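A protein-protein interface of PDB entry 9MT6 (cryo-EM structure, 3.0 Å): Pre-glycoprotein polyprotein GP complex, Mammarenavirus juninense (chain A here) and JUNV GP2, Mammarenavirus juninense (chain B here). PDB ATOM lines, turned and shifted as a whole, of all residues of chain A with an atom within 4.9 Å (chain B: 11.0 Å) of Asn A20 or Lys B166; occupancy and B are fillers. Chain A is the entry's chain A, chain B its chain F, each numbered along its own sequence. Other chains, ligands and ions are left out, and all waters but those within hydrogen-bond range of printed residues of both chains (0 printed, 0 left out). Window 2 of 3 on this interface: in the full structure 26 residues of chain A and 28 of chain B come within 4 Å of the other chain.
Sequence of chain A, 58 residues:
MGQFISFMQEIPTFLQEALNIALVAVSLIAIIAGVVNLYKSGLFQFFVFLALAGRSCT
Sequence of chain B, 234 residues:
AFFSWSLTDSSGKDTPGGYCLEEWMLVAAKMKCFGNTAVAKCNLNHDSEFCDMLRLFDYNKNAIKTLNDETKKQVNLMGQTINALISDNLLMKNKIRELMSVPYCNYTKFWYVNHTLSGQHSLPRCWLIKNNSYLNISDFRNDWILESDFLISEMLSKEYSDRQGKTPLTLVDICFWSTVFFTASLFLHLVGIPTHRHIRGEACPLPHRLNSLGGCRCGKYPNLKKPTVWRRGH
Pro B168 touches Phe A14 (CG to CD2, 3.7 Å). CD2 of Leu A19 touches NH1 of Arg B163, 3.4 Å away. Thr B167 touches Leu A19 (OG1 to CD2, 3.5 Å). O of Lys B166 touches ND2 of Asn A20, 3.6 Å away. Leu B171 touches Asn A20 (CD2 to O, 3.6 Å). CD1 of Leu A23 touches CG2 of Thr B167, 3.97 Å away. Leu A23 touches Leu B171 (CB to CG, 3.8 Å). Leu A23 touches Cys B175 (CD2 to SG, 3.7 Å). Leu B171 touches Val A24 (CD1 to CG2, 3.6 Å).
Asn A20 touches three residues of chain B. Of chain A, only Asn A20 comes within 4 Å of Lys B166. No residue of chain B comes within 4 Å of Glu A17. Ala A18 touches none of the printed residues of chain B. Leu A19 touches two residues of chain B. No residue of chain B comes within 4 Å of Ile A21. No residue of chain B comes within 4 Å of Ala A22. Of chain B, only Leu B171 (3.6 Å) comes within 4 Å of Val A24. Printed residues of chain A within 4 Å of Pro B168: Phe A14. Printed residues of chain A within 4 Å of Thr B167: Leu A19, Asn A20 and Leu A23. Asp B162 touches none of the printed residues of chain A. The nearest residue of chain B that does not touch Asn A20 is Pro B168 (4.1 Å).
The side-chain amide nitrogen (ND2) of Asn A20 is in hydrogen-bond range of the backbone carbonyl oxygen (O) of Phe A14 (2.6 Å).
The side-chain hydroxyl of Thr B167 sits at hydrogen-bond distance from the side-chain amide oxygen of Asn A20 (2.9 Å).
Of the 18 printed residues of chain B, 6 touch a printed residue of chain A. Hydrophobic or aromatic side chains of chain B within 4 Å of the printed part of chain A: Pro B168 and Leu B171. Among the printed residues, 10 pairs touch across the chains. Among the printed residues, no Asp or Glu carboxylate lies within 4 Å of a Lys or Arg side-chain nitrogen of the other chain.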
ATOM      1  N   PHE A  14       5.678  -3.439 -21.163  1.00  0.00           N
ATOM      2  CA  PHE A  14       4.428  -3.308 -21.901  1.00  0.00           C
ATOM      3  C   PHE A  14       3.372  -2.522 -21.136  1.00  0.00           C
ATOM      4  O   PHE A  14       2.537  -1.859 -21.758  1.00  0.00           O
ATOM      5  CB  PHE A  14       3.884  -4.687 -22.269  1.00  0.00           C
ATOM      6  CG  PHE A  14       4.769  -5.455 -23.197  1.00  0.00           C
ATOM      7  CD1 PHE A  14       5.536  -4.797 -24.141  1.00  0.00           C
ATOM      8  CD2 PHE A  14       4.824  -6.834 -23.142  1.00  0.00           C
ATOM      9  CE1 PHE A  14       6.352  -5.497 -25.001  1.00  0.00           C
ATOM     10  CE2 PHE A  14       5.638  -7.542 -24.002  1.00  0.00           C
ATOM     11  CZ  PHE A  14       6.402  -6.873 -24.933  1.00  0.00           C
ATOM     12  N   LEU A  15       3.381  -2.579 -19.804  1.00  0.00           N
ATOM     13  CA  LEU A  15       2.333  -1.924 -19.032  1.00  0.00           C
ATOM     14  C   LEU A  15       2.607  -0.437 -18.851  1.00  0.00           C
ATOM     15  O   LEU A  15       2.562   0.077 -17.729  1.00  0.00           O
ATOM     16  CB  LEU A  15       2.168  -2.587 -17.665  1.00  0.00           C
ATOM     17  CG  LEU A  15       1.967  -4.099 -17.631  1.00  0.00           C
ATOM     18  CD1 LEU A  15       2.264  -4.620 -16.238  1.00  0.00           C
ATOM     19  CD2 LEU A  15       0.559  -4.461 -18.055  1.00  0.00           C
ATOM     20  N   GLU A  17       1.244   1.592 -21.677  1.00  0.00           N
ATOM     21  CA  GLU A  17       0.154   2.082 -22.503  1.00  0.00           C
ATOM     22  C   GLU A  17      -1.175   1.617 -21.925  1.00  0.00           C
ATOM     23  O   GLU A  17      -1.269   0.544 -21.325  1.00  0.00           O
ATOM     24  CB  GLU A  17       0.301   1.596 -23.945  1.00  0.00           C
ATOM     25  CG  GLU A  17       1.520   2.148 -24.664  1.00  0.00           C
ATOM     26  CD  GLU A  17       1.433   3.642 -24.904  1.00  0.00           C
ATOM     27  OE1 GLU A  17       0.309   4.154 -25.087  1.00  0.00           O
ATOM     28  OE2 GLU A  17       2.491   4.306 -24.911  1.00  0.00           O
ATOM     29  N   ALA A  18      -2.206   2.446 -22.101  1.00  0.00           N
ATOM     30  CA  ALA A  18      -3.518   2.112 -21.560  1.00  0.00           C
ATOM     31  C   ALA A  18      -4.080   0.856 -22.211  1.00  0.00           C
ATOM     32  O   ALA A  18      -4.731   0.040 -21.545  1.00  0.00           O
ATOM     33  CB  ALA A  18      -4.475   3.289 -21.745  1.00  0.00           C
ATOM     34  N   LEU A  19      -3.841   0.685 -23.511  1.00  0.00           N
ATOM     35  CA  LEU A  19      -4.398  -0.460 -24.222  1.00  0.00           C
ATOM     36  C   LEU A  19      -3.814  -1.771 -23.714  1.00  0.00           C
ATOM     37  O   LEU A  19      -4.528  -2.774 -23.618  1.00  0.00           O
ATOM     38  CB  LEU A  19      -4.159  -0.308 -25.722  1.00  0.00           C
ATOM     39  CG  LEU A  19      -4.721  -1.412 -26.611  1.00  0.00           C
ATOM     40  CD1 LEU A  19      -6.234  -1.416 -26.565  1.00  0.00           C
ATOM     41  CD2 LEU A  19      -4.231  -1.242 -28.029  1.00  0.00           C
ATOM     42  N   ASN A  20      -2.519  -1.792 -23.395  1.00  0.00           N
ATOM     43  CA  ASN A  20      -1.910  -3.017 -22.884  1.00  0.00           C
ATOM     44  C   ASN A  20      -2.491  -3.401 -21.530  1.00  0.00           C
ATOM     45  O   ASN A  20      -2.769  -4.582 -21.276  1.00  0.00           O
ATOM     46  CB  ASN A  20      -0.397  -2.847 -22.792  1.00  0.00           C
ATOM     47  CG  ASN A  20       0.236  -2.554 -24.131  1.00  0.00           C
ATOM     48  OD1 ASN A  20      -0.430  -2.584 -25.163  1.00  0.00           O
ATOM     49  ND2 ASN A  20       1.529  -2.264 -24.124  1.00  0.00           N
ATOM     50  N   ILE A  21      -2.679  -2.421 -20.645  1.00  0.00           N
ATOM     51  CA  ILE A  21      -3.299  -2.689 -19.351  1.00  0.00           C
ATOM     52  C   ILE A  21      -4.722  -3.188 -19.545  1.00  0.00           C
ATOM     53  O   ILE A  21      -5.172  -4.116 -18.860  1.00  0.00           O
ATOM     54  CB  ILE A  21      -3.259  -1.432 -18.466  1.00  0.00           C
ATOM     55  CG1 ILE A  21      -1.823  -0.937 -18.306  1.00  0.00           C
ATOM     56  CG2 ILE A  21      -3.872  -1.717 -17.107  1.00  0.00           C
ATOM     57  CD1 ILE A  21      -1.714   0.387 -17.596  1.00  0.00           C
ATOM     58  N   ALA A  22      -5.453  -2.577 -20.480  1.00  0.00           N
ATOM     59  CA  ALA A  22      -6.812  -3.019 -20.765  1.00  0.00           C
ATOM     60  C   ALA A  22      -6.831  -4.459 -21.252  1.00  0.00           C
ATOM     61  O   ALA A  22      -7.685  -5.250 -20.841  1.00  0.00           O
ATOM     62  CB  ALA A  22      -7.459  -2.096 -21.795  1.00  0.00           C
ATOM     63  N   LEU A  23      -5.895  -4.815 -22.132  1.00  0.00           N
ATOM     64  CA  LEU A  23      -5.838  -6.178 -22.648  1.00  0.00           C
ATOM     65  C   LEU A  23      -5.508  -7.175 -21.545  1.00  0.00           C
ATOM     66  O   LEU A  23      -6.107  -8.252 -21.477  1.00  0.00           O
ATOM     67  CB  LEU A  23      -4.818  -6.269 -23.782  1.00  0.00           C
ATOM     68  CG  LEU A  23      -5.212  -5.606 -25.103  1.00  0.00           C
ATOM     69  CD1 LEU A  23      -4.142  -5.817 -26.151  1.00  0.00           C
ATOM     70  CD2 LEU A  23      -6.546  -6.127 -25.593  1.00  0.00           C
ATOM     71  N   VAL A  24      -4.562  -6.832 -20.666  1.00  0.00           N
ATOM     72  CA  VAL A  24      -4.219  -7.729 -19.562  1.00  0.00           C
ATOM     73  C   VAL A  24      -5.415  -7.918 -18.636  1.00  0.00           C
ATOM     74  O   VAL A  24      -5.734  -9.041 -18.221  1.00  0.00           O
ATOM     75  CB  VAL A  24      -2.994  -7.200 -18.796  1.00  0.00           C
ATOM     76  CG1 VAL A  24      -2.809  -7.968 -17.500  1.00  0.00           C
ATOM     77  CG2 VAL A  24      -1.750  -7.305 -19.650  1.00  0.00           C
ATOM     78  N   LYS B 158      -0.097   3.844 -41.371  1.00  0.00           N
ATOM     79  CA  LYS B 158       0.733   4.401 -40.312  1.00  0.00           C
ATOM     80  C   LYS B 158       0.071   4.223 -38.958  1.00  0.00           C
ATOM     81  O   LYS B 158       0.746   3.943 -37.961  1.00  0.00           O
ATOM     82  CB  LYS B 158       1.010   5.878 -40.582  1.00  0.00           C
ATOM     83  CG  LYS B 158       1.762   6.574 -39.465  1.00  0.00           C
ATOM     84  CD  LYS B 158       2.218   7.959 -39.885  1.00  0.00           C
ATOM     85  CE  LYS B 158       3.116   8.582 -38.832  1.00  0.00           C
ATOM     86  NZ  LYS B 158       4.040   7.577 -38.235  1.00  0.00           N
ATOM     87  N   GLU B 159      -1.251   4.388 -38.898  1.00  0.00           N
ATOM     88  CA  GLU B 159      -1.951   4.129 -37.643  1.00  0.00           C
ATOM     89  C   GLU B 159      -1.780   2.675 -37.210  1.00  0.00           C
ATOM     90  O   GLU B 159      -1.484   2.392 -36.040  1.00  0.00           O
ATOM     91  CB  GLU B 159      -3.428   4.487 -37.789  1.00  0.00           C
ATOM     92  CG  GLU B 159      -4.226   4.368 -36.510  1.00  0.00           C
ATOM     93  CD  GLU B 159      -5.663   4.808 -36.686  1.00  0.00           C
ATOM     94  OE1 GLU B 159      -6.036   5.184 -37.817  1.00  0.00           O
ATOM     95  OE2 GLU B 159      -6.422   4.775 -35.694  1.00  0.00           O
ATOM     96  N   TYR B 160      -1.928   1.740 -38.153  1.00  0.00           N
ATOM     97  CA  TYR B 160      -1.728   0.328 -37.830  1.00  0.00           C
ATOM     98  C   TYR B 160      -0.302   0.050 -37.366  1.00  0.00           C
ATOM     99  O   TYR B 160      -0.089  -0.704 -36.411  1.00  0.00           O
ATOM    100  CB  TYR B 160      -2.068  -0.547 -39.035  1.00  0.00           C
ATOM    101  CG  TYR B 160      -3.497  -1.032 -39.080  1.00  0.00           C
ATOM    102  CD1 TYR B 160      -3.895  -2.138 -38.350  1.00  0.00           C
ATOM    103  CD2 TYR B 160      -4.441  -0.394 -39.866  1.00  0.00           C
ATOM    104  CE1 TYR B 160      -5.197  -2.590 -38.395  1.00  0.00           C
ATOM    105  CE2 TYR B 160      -5.746  -0.838 -39.915  1.00  0.00           C
ATOM    106  CZ  TYR B 160      -6.118  -1.937 -39.179  1.00  0.00           C
ATOM    107  OH  TYR B 160      -7.418  -2.382 -39.227  1.00  0.00           O
ATOM    108  N   SER B 161       0.689   0.637 -38.039  1.00  0.00           N
ATOM    109  CA  SER B 161       2.083   0.406 -37.672  1.00  0.00           C
ATOM    110  C   SER B 161       2.397   0.980 -36.297  1.00  0.00           C
ATOM    111  O   SER B 161       3.134   0.366 -35.516  1.00  0.00           O
ATOM    112  CB  SER B 161       3.008   1.006 -38.726  1.00  0.00           C
ATOM    113  OG  SER B 161       3.173   2.398 -38.522  1.00  0.00           O
ATOM    114  N   ASP B 162       1.858   2.160 -35.989  1.00  0.00           N
ATOM    115  CA  ASP B 162       2.045   2.737 -34.663  1.00  0.00           C
ATOM    116  C   ASP B 162       1.421   1.858 -33.593  1.00  0.00           C
ATOM    117  O   ASP B 162       1.972   1.716 -32.495  1.00  0.00           O
ATOM    118  CB  ASP B 162       1.455   4.145 -34.615  1.00  0.00           C
ATOM    119  CG  ASP B 162       2.273   5.143 -35.402  1.00  0.00           C
ATOM    120  OD1 ASP B 162       3.276   4.731 -36.022  1.00  0.00           O
ATOM    121  OD2 ASP B 162       1.913   6.338 -35.402  1.00  0.00           O
ATOM    122  N   ARG B 163       0.259   1.268 -33.886  1.00  0.00           N
ATOM    123  CA  ARG B 163      -0.316   0.292 -32.964  1.00  0.00           C
ATOM    124  C   ARG B 163       0.607  -0.904 -32.778  1.00  0.00           C
ATOM    125  O   ARG B 163       0.854  -1.342 -31.649  1.00  0.00           O
ATOM    126  CB  ARG B 163      -1.684  -0.165 -33.463  1.00  0.00           C
ATOM    127  CG  ARG B 163      -2.288  -1.283 -32.636  1.00  0.00           C
ATOM    128  CD  ARG B 163      -2.541  -0.853 -31.210  1.00  0.00           C
ATOM    129  NE  ARG B 163      -3.496   0.242 -31.129  1.00  0.00           N
ATOM    130  CZ  ARG B 163      -4.811   0.086 -31.139  1.00  0.00           C
ATOM    131  NH1 ARG B 163      -5.363  -1.109 -31.244  1.00  0.00           N
ATOM    132  NH2 ARG B 163      -5.592   1.157 -31.040  1.00  0.00           N
ATOM    133  N   GLN B 164       1.125  -1.448 -33.879  1.00  0.00           N
ATOM    134  CA  GLN B 164       1.935  -2.659 -33.800  1.00  0.00           C
ATOM    135  C   GLN B 164       3.283  -2.424 -33.136  1.00  0.00           C
ATOM    136  O   GLN B 164       3.878  -3.376 -32.623  1.00  0.00           O
ATOM    137  CB  GLN B 164       2.138  -3.250 -35.195  1.00  0.00           C
ATOM    138  CG  GLN B 164       0.860  -3.767 -35.825  1.00  0.00           C
ATOM    139  CD  GLN B 164       1.061  -4.270 -37.235  1.00  0.00           C
ATOM    140  OE1 GLN B 164       2.151  -4.168 -37.794  1.00  0.00           O
ATOM    141  NE2 GLN B 164       0.005  -4.818 -37.821  1.00  0.00           N
ATOM    142  N   GLY B 165       3.781  -1.191 -33.136  1.00  0.00           N
ATOM    143  CA  GLY B 165       5.039  -0.911 -32.474  1.00  0.00           C
ATOM    144  C   GLY B 165       4.955  -0.733 -30.975  1.00  0.00           C
ATOM    145  O   GLY B 165       5.994  -0.667 -30.314  1.00  0.00           O
ATOM    146  N   LYS B 166       3.749  -0.659 -30.425  1.00  0.00           N
ATOM    147  CA  LYS B 166       3.539  -0.488 -28.993  1.00  0.00           C
ATOM    148  C   LYS B 166       2.913  -1.702 -28.332  1.00  0.00           C
ATOM    149  O   LYS B 166       3.358  -2.109 -27.258  1.00  0.00           O
ATOM    150  CB  LYS B 166       2.653   0.735 -28.730  1.00  0.00           C
ATOM    151  CG  LYS B 166       3.218   2.041 -29.250  1.00  0.00           C
ATOM    152  CD  LYS B 166       2.241   3.185 -29.042  1.00  0.00           C
ATOM    153  CE  LYS B 166       0.847   2.821 -29.526  1.00  0.00           C
ATOM    154  NZ  LYS B 166      -0.052   4.007 -29.562  1.00  0.00           N
ATOM    155  N   THR B 167       1.894  -2.293 -28.947  1.00  0.00           N
ATOM    156  CA  THR B 167       1.185  -3.417 -28.356  1.00  0.00           C
ATOM    157  C   THR B 167       1.784  -4.723 -28.854  1.00  0.00           C
ATOM    158  O   THR B 167       1.841  -4.939 -30.071  1.00  0.00           O
ATOM    159  CB  THR B 167      -0.293  -3.360 -28.700  1.00  0.00           C
ATOM    160  OG1 THR B 167      -0.892  -2.235 -28.046  1.00  0.00           O
ATOM    161  CG2 THR B 167      -0.996  -4.626 -28.250  1.00  0.00           C
ATOM    162  N   PRO B 168       2.245  -5.605 -27.971  1.00  0.00           N
ATOM    163  CA  PRO B 168       2.810  -6.876 -28.424  1.00  0.00           C
ATOM    164  C   PRO B 168       1.759  -7.780 -29.045  1.00  0.00           C
ATOM    165  O   PRO B 168       0.572  -7.719 -28.712  1.00  0.00           O
ATOM    166  CB  PRO B 168       3.374  -7.487 -27.138  1.00  0.00           C
ATOM    167  CG  PRO B 168       2.574  -6.873 -26.058  1.00  0.00           C
ATOM    168  CD  PRO B 168       2.286  -5.476 -26.507  1.00  0.00           C
ATOM    169  N   LEU B 169       2.215  -8.631 -29.965  1.00  0.00           N
ATOM    170  CA  LEU B 169       1.316  -9.581 -30.611  1.00  0.00           C
ATOM    171  C   LEU B 169       0.870 -10.664 -29.641  1.00  0.00           C
ATOM    172  O   LEU B 169      -0.271 -11.139 -29.710  1.00  0.00           O
ATOM    173  CB  LEU B 169       1.998 -10.202 -31.828  1.00  0.00           C
ATOM    174  CG  LEU B 169       1.294 -11.381 -32.493  1.00  0.00           C
ATOM    175  CD1 LEU B 169       0.170 -10.901 -33.384  1.00  0.00           C
ATOM    176  CD2 LEU B 169       2.289 -12.208 -33.277  1.00  0.00           C
ATOM    177  N   THR B 170       1.758 -11.073 -28.734  1.00  0.00           N
ATOM    178  CA  THR B 170       1.423 -12.133 -27.791  1.00  0.00           C
ATOM    179  C   THR B 170       0.278 -11.718 -26.880  1.00  0.00           C
ATOM    180  O   THR B 170      -0.585 -12.534 -26.546  1.00  0.00           O
ATOM    181  CB  THR B 170       2.653 -12.513 -26.970  1.00  0.00           C
ATOM    182  OG1 THR B 170       3.696 -12.944 -27.852  1.00  0.00           O
ATOM    183  CG2 THR B 170       2.325 -13.637 -26.007  1.00  0.00           C
ATOM    184  N   LEU B 171       0.250 -10.450 -26.469  1.00  0.00           N
ATOM    185  CA  LEU B 171      -0.840  -9.973 -25.626  1.00  0.00           C
ATOM    186  C   LEU B 171      -2.163  -9.974 -26.382  1.00  0.00           C
ATOM    187  O   LEU B 171      -3.207 -10.331 -25.821  1.00  0.00           O
ATOM    188  CB  LEU B 171      -0.507  -8.582 -25.095  1.00  0.00           C
ATOM    189  CG  LEU B 171      -1.482  -7.973 -24.101  1.00  0.00           C
ATOM    190  CD1 LEU B 171      -1.571  -8.859 -22.881  1.00  0.00           C
ATOM    191  CD2 LEU B 171      -1.016  -6.587 -23.714  1.00  0.00           C
ATOM    192  N   VAL B 172      -2.135  -9.598 -27.663  1.00  0.00           N
ATOM    193  CA  VAL B 172      -3.339  -9.652 -28.489  1.00  0.00           C
ATOM    194  C   VAL B 172      -3.831 -11.087 -28.615  1.00  0.00           C
ATOM    195  O   VAL B 172      -5.034 -11.362 -28.498  1.00  0.00           O
ATOM    196  CB  VAL B 172      -3.064  -9.026 -29.868  1.00  0.00           C
ATOM    197  CG1 VAL B 172      -4.202  -9.322 -30.826  1.00  0.00           C
ATOM    198  CG2 VAL B 172      -2.846  -7.533 -29.736  1.00  0.00           C
ATOM    199  N   ASP B 173      -2.911 -12.023 -28.855  1.00  0.00           N
ATOM    200  CA  ASP B 173      -3.291 -13.427 -28.965  1.00  0.00           C
ATOM    201  C   ASP B 173      -3.863 -13.948 -27.654  1.00  0.00           C
ATOM    202  O   ASP B 173      -4.849 -14.694 -27.649  1.00  0.00           O
ATOM    203  CB  ASP B 173      -2.086 -14.263 -29.389  1.00  0.00           C
ATOM    204  CG  ASP B 173      -1.926 -14.333 -30.892  1.00  0.00           C
ATOM    205  OD1 ASP B 173      -2.839 -13.876 -31.611  1.00  0.00           O
ATOM    206  OD2 ASP B 173      -0.888 -14.849 -31.354  1.00  0.00           O
ATOM    207  N   ILE B 174      -3.251 -13.570 -26.531  1.00  0.00           N
ATOM    208  CA  ILE B 174      -3.741 -13.996 -25.226  1.00  0.00           C
ATOM    209  C   ILE B 174      -5.152 -13.478 -24.996  1.00  0.00           C
ATOM    210  O   ILE B 174      -6.029 -14.213 -24.531  1.00  0.00           O
ATOM    211  CB  ILE B 174      -2.777 -13.535 -24.118  1.00  0.00           C
ATOM    212  CG1 ILE B 174      -1.545 -14.436 -24.076  1.00  0.00           C
ATOM    213  CG2 ILE B 174      -3.469 -13.533 -22.771  1.00  0.00           C
ATOM    214  CD1 ILE B 174      -0.428 -13.895 -23.217  1.00  0.00           C
ATOM    215  N   CYS B 175      -5.397 -12.208 -25.325  1.00  0.00           N
ATOM    216  CA  CYS B 175      -6.737 -11.654 -25.155  1.00  0.00           C
ATOM    217  C   CYS B 175      -7.750 -12.366 -26.044  1.00  0.00           C
ATOM    218  O   CYS B 175      -8.856 -12.694 -25.597  1.00  0.00           O
ATOM    219  CB  CYS B 175      -6.727 -10.156 -25.444  1.00  0.00           C
ATOM    220  SG  CYS B 175      -8.279  -9.322 -25.074  1.00  0.00           S
